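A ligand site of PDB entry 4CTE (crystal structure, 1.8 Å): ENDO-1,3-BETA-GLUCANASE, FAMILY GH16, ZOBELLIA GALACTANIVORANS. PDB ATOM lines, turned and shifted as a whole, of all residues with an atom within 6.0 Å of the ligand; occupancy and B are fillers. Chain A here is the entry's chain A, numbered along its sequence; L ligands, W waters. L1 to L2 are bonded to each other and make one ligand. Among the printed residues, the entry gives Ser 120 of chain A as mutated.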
ATOM      1  N   TRP A  30       1.101 -26.838  18.654  1.00  0.00           N
ATOM      2  CA  TRP A  30       2.129 -27.294  17.689  1.00  0.00           C
ATOM      3  C   TRP A  30       3.379 -27.787  18.386  1.00  0.00           C
ATOM      4  O   TRP A  30       4.485 -27.537  17.941  1.00  0.00           O
ATOM      5  CB  TRP A  30       2.386 -26.180  16.638  1.00  0.00           C
ATOM      6  CG  TRP A  30       1.112 -26.011  15.844  1.00  0.00           C
ATOM      7  CD1 TRP A  30       0.056 -25.115  16.064  1.00  0.00           C
ATOM      8  CD2 TRP A  30       0.697 -26.827  14.713  1.00  0.00           C
ATOM      9  NE1 TRP A  30      -0.944 -25.316  15.167  1.00  0.00           N
ATOM     10  CE2 TRP A  30      -0.630 -26.325  14.318  1.00  0.00           C
ATOM     11  CE3 TRP A  30       1.273 -27.887  13.999  1.00  0.00           C
ATOM     12  CZ2 TRP A  30      -1.339 -26.880  13.220  1.00  0.00           C
ATOM     13  CZ3 TRP A  30       0.557 -28.423  12.892  1.00  0.00           C
ATOM     14  CH2 TRP A  30      -0.731 -27.943  12.546  1.00  0.00           C
ATOM     15  N   GLY A  31       3.184 -28.456  19.544  1.00  0.00           N
ATOM     16  CA  GLY A  31       4.273 -29.039  20.324  1.00  0.00           C
ATOM     17  C   GLY A  31       5.076 -28.034  21.119  1.00  0.00           C
ATOM     18  O   GLY A  31       5.977 -28.429  21.865  1.00  0.00           O
ATOM     19  N   ASN A  32       4.737 -26.747  21.008  1.00  0.00           N
ATOM     20  CA  ASN A  32       5.484 -25.701  21.686  1.00  0.00           C
ATOM     21  C   ASN A  32       4.667 -24.720  22.504  1.00  0.00           C
ATOM     22  O   ASN A  32       5.176 -23.633  22.765  1.00  0.00           O
ATOM     23  CB  ASN A  32       6.294 -24.913  20.656  1.00  0.00           C
ATOM     24  CG  ASN A  32       7.323 -25.756  19.939  1.00  0.00           C
ATOM     25  OD1 ASN A  32       7.294 -25.866  18.715  1.00  0.00           O
ATOM     26  ND2 ASN A  32       8.221 -26.366  20.677  1.00  0.00           N
ATOM     27  N   GLU A  34       2.260 -22.923  21.581  1.00  0.00           N
ATOM     28  CA  GLU A  34       1.985 -21.723  20.770  1.00  0.00           C
ATOM     29  C   GLU A  34       0.537 -21.256  20.975  1.00  0.00           C
ATOM     30  O   GLU A  34      -0.377 -22.057  21.322  1.00  0.00           O
ATOM     31  CB  GLU A  34       2.269 -21.960  19.294  1.00  0.00           C
ATOM     32  CG  GLU A  34       3.745 -22.190  19.079  1.00  0.00           C
ATOM     33  CD  GLU A  34       4.097 -22.900  17.783  1.00  0.00           C
ATOM     34  OE1 GLU A  34       3.295 -22.889  16.813  1.00  0.00           O
ATOM     35  OE2 GLU A  34       5.207 -23.448  17.753  1.00  0.00           O
ATOM     36  N   ARG A  68       0.197 -21.420   8.609  1.00  0.00           N
ATOM     37  CA  ARG A  68       1.281 -22.371   8.514  1.00  0.00           C
ATOM     38  C   ARG A  68       1.009 -23.161   7.244  1.00  0.00           C
ATOM     39  O   ARG A  68      -0.108 -23.724   7.030  1.00  0.00           O
ATOM     40  CB  ARG A  68       1.318 -23.286   9.701  1.00  0.00           C
ATOM     41  CG  ARG A  68       2.350 -24.407   9.603  1.00  0.00           C
ATOM     42  CD  ARG A  68       2.601 -24.998  10.977  1.00  0.00           C
ATOM     43  NE  ARG A  68       3.161 -26.349  10.941  1.00  0.00           N
ATOM     44  CZ  ARG A  68       3.864 -26.915  11.924  1.00  0.00           C
ATOM     45  NH1 ARG A  68       4.168 -26.228  13.045  1.00  0.00           N
ATOM     46  NH2 ARG A  68       4.279 -28.185  11.795  1.00  0.00           N
ATOM     47  N   TRP A  95       6.895 -15.284  16.140  1.00  0.00           N
ATOM     48  CA  TRP A  95       7.885 -16.314  15.929  1.00  0.00           C
ATOM     49  C   TRP A  95       7.798 -16.907  14.554  1.00  0.00           C
ATOM     50  O   TRP A  95       7.308 -18.049  14.389  1.00  0.00           O
ATOM     51  CB  TRP A  95       7.747 -17.404  16.981  1.00  0.00           C
ATOM     52  CG  TRP A  95       8.692 -18.571  16.779  1.00  0.00           C
ATOM     53  CD1 TRP A  95       9.766 -18.651  15.895  1.00  0.00           C
ATOM     54  CD2 TRP A  95       8.693 -19.858  17.493  1.00  0.00           C
ATOM     55  NE1 TRP A  95      10.396 -19.858  16.001  1.00  0.00           N
ATOM     56  CE2 TRP A  95       9.807 -20.628  16.942  1.00  0.00           C
ATOM     57  CE3 TRP A  95       7.904 -20.418  18.482  1.00  0.00           C
ATOM     58  CZ2 TRP A  95      10.101 -21.906  17.375  1.00  0.00           C
ATOM     59  CZ3 TRP A  95       8.215 -21.713  18.923  1.00  0.00           C
ATOM     60  CH2 TRP A  95       9.289 -22.434  18.376  1.00  0.00           C
ATOM     61  N   PRO A  96       8.262 -16.170  13.561  1.00  0.00           N
ATOM     62  CA  PRO A  96       8.264 -16.686  12.193  1.00  0.00           C
ATOM     63  C   PRO A  96       9.327 -17.796  11.985  1.00  0.00           C
ATOM     64  O   PRO A  96      10.351 -17.841  12.720  1.00  0.00           O
ATOM     65  CB  PRO A  96       8.637 -15.474  11.401  1.00  0.00           C
ATOM     66  CG  PRO A  96       9.621 -14.756  12.331  1.00  0.00           C
ATOM     67  CD  PRO A  96       8.912 -14.851  13.640  1.00  0.00           C
ATOM     68  N   ALA A  97       9.102 -18.645  10.980  1.00  0.00           N
ATOM     69  CA  ALA A  97      10.069 -19.720  10.675  1.00  0.00           C
ATOM     70  C   ALA A  97       9.952 -20.147   9.244  1.00  0.00           C
ATOM     71  O   ALA A  97       8.869 -20.128   8.678  1.00  0.00           O
ATOM     72  CB  ALA A  97       9.895 -20.930  11.597  1.00  0.00           C
ATOM     73  N   TRP A  99      11.501 -23.463   7.363  1.00  0.00           N
ATOM     74  CA  TRP A  99      12.106 -24.689   7.829  1.00  0.00           C
ATOM     75  C   TRP A  99      11.702 -25.895   7.046  1.00  0.00           C
ATOM     76  O   TRP A  99      10.937 -25.785   6.094  1.00  0.00           O
ATOM     77  CB  TRP A  99      11.792 -24.821   9.334  1.00  0.00           C
ATOM     78  CG  TRP A  99      10.344 -24.790   9.733  1.00  0.00           C
ATOM     79  CD1 TRP A  99       9.412 -23.764   9.512  1.00  0.00           C
ATOM     80  CD2 TRP A  99       9.666 -25.769  10.586  1.00  0.00           C
ATOM     81  NE1 TRP A  99       8.213 -24.065  10.133  1.00  0.00           N
ATOM     82  CE2 TRP A  99       8.298 -25.260  10.784  1.00  0.00           C
ATOM     83  CE3 TRP A  99      10.044 -26.999  11.203  1.00  0.00           C
ATOM     84  CZ2 TRP A  99       7.363 -25.954  11.552  1.00  0.00           C
ATOM     85  CZ3 TRP A  99       9.087 -27.692  11.971  1.00  0.00           C
ATOM     86  CH2 TRP A  99       7.772 -27.179  12.129  1.00  0.00           C
ATOM     87  N   LEU A 101      11.149 -30.431   7.306  1.00  0.00           N
ATOM     88  CA  LEU A 101      10.950 -31.647   8.057  1.00  0.00           C
ATOM     89  C   LEU A 101      11.085 -32.829   7.153  1.00  0.00           C
ATOM     90  O   LEU A 101      10.699 -32.738   5.988  1.00  0.00           O
ATOM     91  CB  LEU A 101       9.552 -31.680   8.681  1.00  0.00           C
ATOM     92  CG  LEU A 101       9.293 -30.788   9.892  1.00  0.00           C
ATOM     93  CD1 LEU A 101       7.786 -30.791  10.178  1.00  0.00           C
ATOM     94  CD2 LEU A 101      10.088 -31.222  11.127  1.00  0.00           C
ATOM     95  N   ILE A 105       8.381 -38.250   8.701  1.00  0.00           N
ATOM     96  CA  ILE A 105       7.689 -37.794   9.926  1.00  0.00           C
ATOM     97  C   ILE A 105       6.456 -38.677  10.167  1.00  0.00           C
ATOM     98  O   ILE A 105       6.143 -38.982  11.316  1.00  0.00           O
ATOM     99  CB  ILE A 105       7.344 -36.254   9.968  1.00  0.00           C
ATOM    100  CG1 ILE A 105       7.008 -35.820  11.420  1.00  0.00           C
ATOM    101  CG2 ILE A 105       6.265 -35.820   8.964  1.00  0.00           C
ATOM    102  CD1 ILE A 105       6.957 -34.334  11.667  1.00  0.00           C
ATOM    103  N   TRP A 110       8.660 -37.041  15.265  1.00  0.00           N
ATOM    104  CA  TRP A 110       9.625 -35.970  15.513  1.00  0.00           C
ATOM    105  C   TRP A 110      10.315 -36.196  16.857  1.00  0.00           C
ATOM    106  O   TRP A 110       9.636 -36.592  17.799  1.00  0.00           O
ATOM    107  CB  TRP A 110       8.884 -34.615  15.440  1.00  0.00           C
ATOM    108  CG  TRP A 110       9.799 -33.438  15.597  1.00  0.00           C
ATOM    109  CD1 TRP A 110      10.379 -32.667  14.606  1.00  0.00           C
ATOM    110  CD2 TRP A 110      10.318 -32.874  16.867  1.00  0.00           C
ATOM    111  NE1 TRP A 110      11.184 -31.704  15.146  1.00  0.00           N
ATOM    112  CE2 TRP A 110      11.203 -31.769  16.486  1.00  0.00           C
ATOM    113  CE3 TRP A 110      10.151 -33.184  18.226  1.00  0.00           C
ATOM    114  CZ2 TRP A 110      11.886 -30.997  17.442  1.00  0.00           C
ATOM    115  CZ3 TRP A 110      10.850 -32.396  19.194  1.00  0.00           C
ATOM    116  CH2 TRP A 110      11.695 -31.328  18.809  1.00  0.00           C
ATOM    117  N   GLU A 115      14.931 -32.219  11.286  1.00  0.00           N
ATOM    118  CA  GLU A 115      14.350 -30.910  11.088  1.00  0.00           C
ATOM    119  C   GLU A 115      15.459 -29.950  10.774  1.00  0.00           C
ATOM    120  O   GLU A 115      16.458 -29.928  11.495  1.00  0.00           O
ATOM    121  CB  GLU A 115      13.573 -30.458  12.353  1.00  0.00           C
ATOM    122  CG  GLU A 115      13.125 -29.003  12.307  1.00  0.00           C
ATOM    123  CD  GLU A 115      12.299 -28.531  13.494  1.00  0.00           C
ATOM    124  OE1 GLU A 115      11.746 -29.328  14.282  1.00  0.00           O
ATOM    125  OE2 GLU A 115      12.168 -27.301  13.599  1.00  0.00           O
ATOM    126  N   ASP A 117      15.817 -25.988  10.426  1.00  0.00           N
ATOM    127  CA  ASP A 117      15.324 -24.603  10.615  1.00  0.00           C
ATOM    128  C   ASP A 117      16.282 -23.716   9.844  1.00  0.00           C
ATOM    129  O   ASP A 117      17.416 -23.470  10.312  1.00  0.00           O
ATOM    130  CB  ASP A 117      15.240 -24.216  12.113  1.00  0.00           C
ATOM    131  CG  ASP A 117      14.361 -25.170  12.899  1.00  0.00           C
ATOM    132  OD1 ASP A 117      13.396 -25.741  12.342  1.00  0.00           O
ATOM    133  OD2 ASP A 117      14.617 -25.369  14.105  1.00  0.00           O
ATOM    134  N   MET A 119      15.604 -20.529   8.881  1.00  0.00           N
ATOM    135  CA  MET A 119      15.500 -19.276   9.590  1.00  0.00           C
ATOM    136  C   MET A 119      14.419 -19.383  10.618  1.00  0.00           C
ATOM    137  O   MET A 119      13.295 -19.808  10.285  1.00  0.00           O
ATOM    138  CB  MET A 119      15.173 -18.124   8.615  1.00  0.00           C
ATOM    139  CG  MET A 119      15.028 -16.728   9.225  1.00  0.00           C
ATOM    140  SD  MET A 119      13.496 -16.376  10.143  1.00  0.00           S
ATOM    141  CE  MET A 119      12.226 -16.432   8.859  1.00  0.00           C
ATOM    142  N   SER A 120      14.733 -18.980  11.846  1.00  0.00           N
ATOM    143  CA  SER A 120      13.684 -18.696  12.847  1.00  0.00           C
ATOM    144  C   SER A 120      14.125 -17.443  13.624  1.00  0.00           C
ATOM    145  O   SER A 120      15.332 -17.103  13.698  1.00  0.00           O
ATOM    146  CB  SER A 120      13.376 -19.861  13.763  1.00  0.00           C
ATOM    147  OG  SER A 120      14.527 -20.212  14.502  1.00  0.00           O
ATOM    148  N   HIS A 133      17.278 -30.302  14.391  1.00  0.00           N
ATOM    149  CA  HIS A 133      16.797 -31.141  15.486  1.00  0.00           C
ATOM    150  C   HIS A 133      16.758 -32.540  14.956  1.00  0.00           C
ATOM    151  O   HIS A 133      16.375 -32.739  13.796  1.00  0.00           O
ATOM    152  CB  HIS A 133      15.419 -30.714  15.978  1.00  0.00           C
ATOM    153  CG  HIS A 133      15.352 -29.287  16.461  1.00  0.00           C
ATOM    154  ND1 HIS A 133      15.457 -28.962  17.772  1.00  0.00           N
ATOM    155  CD2 HIS A 133      15.213 -28.087  15.760  1.00  0.00           C
ATOM    156  CE1 HIS A 133      15.387 -27.613  17.897  1.00  0.00           C
ATOM    157  NE2 HIS A 133      15.234 -27.093  16.667  1.00  0.00           N
ATOM    158  N   LEU A 199       8.393 -25.865   5.123  1.00  0.00           N
ATOM    159  CA  LEU A 199       7.299 -25.187   5.836  1.00  0.00           C
ATOM    160  C   LEU A 199       7.580 -23.691   5.952  1.00  0.00           C
ATOM    161  O   LEU A 199       8.756 -23.244   6.026  1.00  0.00           O
ATOM    162  CB  LEU A 199       7.065 -25.774   7.243  1.00  0.00           C
ATOM    163  CG  LEU A 199       6.817 -27.292   7.406  1.00  0.00           C
ATOM    164  CD1 LEU A 199       8.144 -28.026   7.510  1.00  0.00           C
ATOM    165  CD2 LEU A 199       5.910 -27.563   8.621  1.00  0.00           C
ATOM    166  N   ASN A 201       5.739 -20.489   8.357  1.00  0.00           N
ATOM    167  CA  ASN A 201       4.692 -20.090   9.278  1.00  0.00           C
ATOM    168  C   ASN A 201       5.096 -18.887  10.101  1.00  0.00           C
ATOM    169  O   ASN A 201       6.296 -18.467  10.092  1.00  0.00           O
ATOM    170  CB  ASN A 201       4.367 -21.244  10.235  1.00  0.00           C
ATOM    171  CG  ASN A 201       5.490 -21.456  11.237  1.00  0.00           C
ATOM    172  OD1 ASN A 201       6.509 -22.023  10.894  1.00  0.00           O
ATOM    173  ND2 ASN A 201       5.309 -20.965  12.463  1.00  0.00           N
ATOM    174  N   TRP A 208       9.535 -20.829  23.058  1.00  0.00           N
ATOM    175  CA  TRP A 208      10.703 -20.044  22.668  1.00  0.00           C
ATOM    176  C   TRP A 208      10.502 -18.519  22.788  1.00  0.00           C
ATOM    177  O   TRP A 208      11.233 -17.888  23.592  1.00  0.00           O
ATOM    178  CB  TRP A 208      11.217 -20.557  21.309  1.00  0.00           C
ATOM    179  CG  TRP A 208      12.603 -20.039  20.986  1.00  0.00           C
ATOM    180  CD1 TRP A 208      13.637 -19.675  21.887  1.00  0.00           C
ATOM    181  CD2 TRP A 208      13.172 -19.888  19.662  1.00  0.00           C
ATOM    182  NE1 TRP A 208      14.748 -19.252  21.206  1.00  0.00           N
ATOM    183  CE2 TRP A 208      14.551 -19.363  19.863  1.00  0.00           C
ATOM    184  CE3 TRP A 208      12.701 -20.097  18.352  1.00  0.00           C
ATOM    185  CZ2 TRP A 208      15.380 -19.070  18.791  1.00  0.00           C
ATOM    186  CZ3 TRP A 208      13.549 -19.796  17.280  1.00  0.00           C
ATOM    187  CH2 TRP A 208      14.862 -19.297  17.489  1.00  0.00           C
HETATM  188  C1  LIG L   1      12.134 -25.017  17.516  1.00  0.00           C
HETATM  189  S1  LIG L   1      12.462 -24.170  19.021  1.00  0.00           S
HETATM  190  C2  LIG L   1      11.123 -26.119  17.807  1.00  0.00           C
HETATM  191  O1  LIG L   1      11.570 -27.132  18.713  1.00  0.00           O
HETATM  192  C3  LIG L   1      11.026 -26.774  16.488  1.00  0.00           C
HETATM  193  C4  LIG L   1      10.284 -25.757  15.713  1.00  0.00           C
HETATM  194  O2  LIG L   1       9.769 -26.485  14.630  1.00  0.00           O
HETATM  195  C5  LIG L   1      11.360 -24.760  15.322  1.00  0.00           C
HETATM  196  O3  LIG L   1      11.630 -24.074  16.553  1.00  0.00           O
HETATM  197  C6  LIG L   1      10.951 -23.882  14.143  1.00  0.00           C
HETATM  198  O4  LIG L   1      11.491 -22.600  14.411  1.00  0.00           O
HETATM  199  C1  LG2 L   2       8.704 -28.928  16.755  1.00  0.00           C
HETATM  200  S1  LG2 L   2       9.454 -27.303  16.729  1.00  0.00           S
HETATM  201  C2  LG2 L   2       7.968 -29.261  18.084  1.00  0.00           C
HETATM  202  O1  LG2 L   2       8.855 -29.144  19.195  1.00  0.00           O
HETATM  203  C3  LG2 L   2       7.445 -30.708  17.943  1.00  0.00           C
HETATM  204  O2  LG2 L   2       6.808 -31.209  19.168  1.00  0.00           O
HETATM  205  C4  LG2 L   2       6.604 -30.874  16.608  1.00  0.00           C
HETATM  206  O3  LG2 L   2       6.219 -32.233  16.434  1.00  0.00           O
HETATM  207  C5  LG2 L   2       7.383 -30.379  15.342  1.00  0.00           C
HETATM  208  O4  LG2 L   2       7.838 -29.010  15.577  1.00  0.00           O
HETATM  209  C6  LG2 L   2       6.667 -30.505  13.969  1.00  0.00           C
HETATM  210  O5  LG2 L   2       5.558 -29.612  13.868  1.00  0.00           O
HETATM  211  O   HOH W   1       5.563 -27.269  15.271  1.00  0.00           O
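The side-chain carboxylate (OE2) of Glu 115 lies within hydrogen-bond range of an oxygen (O2) of LIG L1 (2.7 Å).
The indole nitrogen of Trp 95 lies close to an oxygen (O4) of LIG L1 (3.4 Å).
O5 of LG2 L2 sits at hydrogen-bond distance from NH2 of Arg 68, at 2.8 Å.
ND2 of Asn 32 sits at hydrogen-bond distance from O1 of LG2 L2, at 3.2 Å.
OE1 of Glu 115 sits at hydrogen-bond distance from NE1 of Trp 110, 2.6 Å away.
The backbone carbonyl oxygen (O) of His 133 sits at hydrogen-bond distance from the backbone NH (N) of Glu 115 (2.9 Å).
The backbone carbonyl oxygen of Trp 99 sits at hydrogen-bond distance from the backbone NH of Leu 199 (2.7 Å).
The side-chain amide oxygen (OD1) of Asn 201 is in hydrogen-bond range of the indole nitrogen (NE1) of Trp 99.
The side-chain amide oxygen (OD1) of Asn 32 sits close to the backbone carbonyl oxygen (O) of Trp 30 (3.4 Å).
The side-chain carboxylate (OE2) of Glu 34 sits close to the side-chain amide oxygen (OD1) of Asn 32 (3.3 Å).
A ring nitrogen (NE2) of His 133 lies within hydrogen-bond range of the side-chain carboxylate (OD2) of Asp 117 (3.1 Å).
The backbone NH of Ala 97 lies within hydrogen-bond range of the backbone carbonyl oxygen of Asn 201 (2.9 Å).
Merely in contact with the ligand: Trp 99, Ser 120, Asp 117, Gly 31, Trp 110, Ala 97, His 133, Trp 30 and Leu 101.
Of the 20 residues printed, 13 come within 4 Å of the ligand.
Water W1 lies within hydrogen-bond range of an oxygen (O5) of LG2 L2 (2.7 Å), the guanidinium group of Arg 68 (2.8 Å) and the backbone carbonyl oxygen of Trp 30 (2.9 Å).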
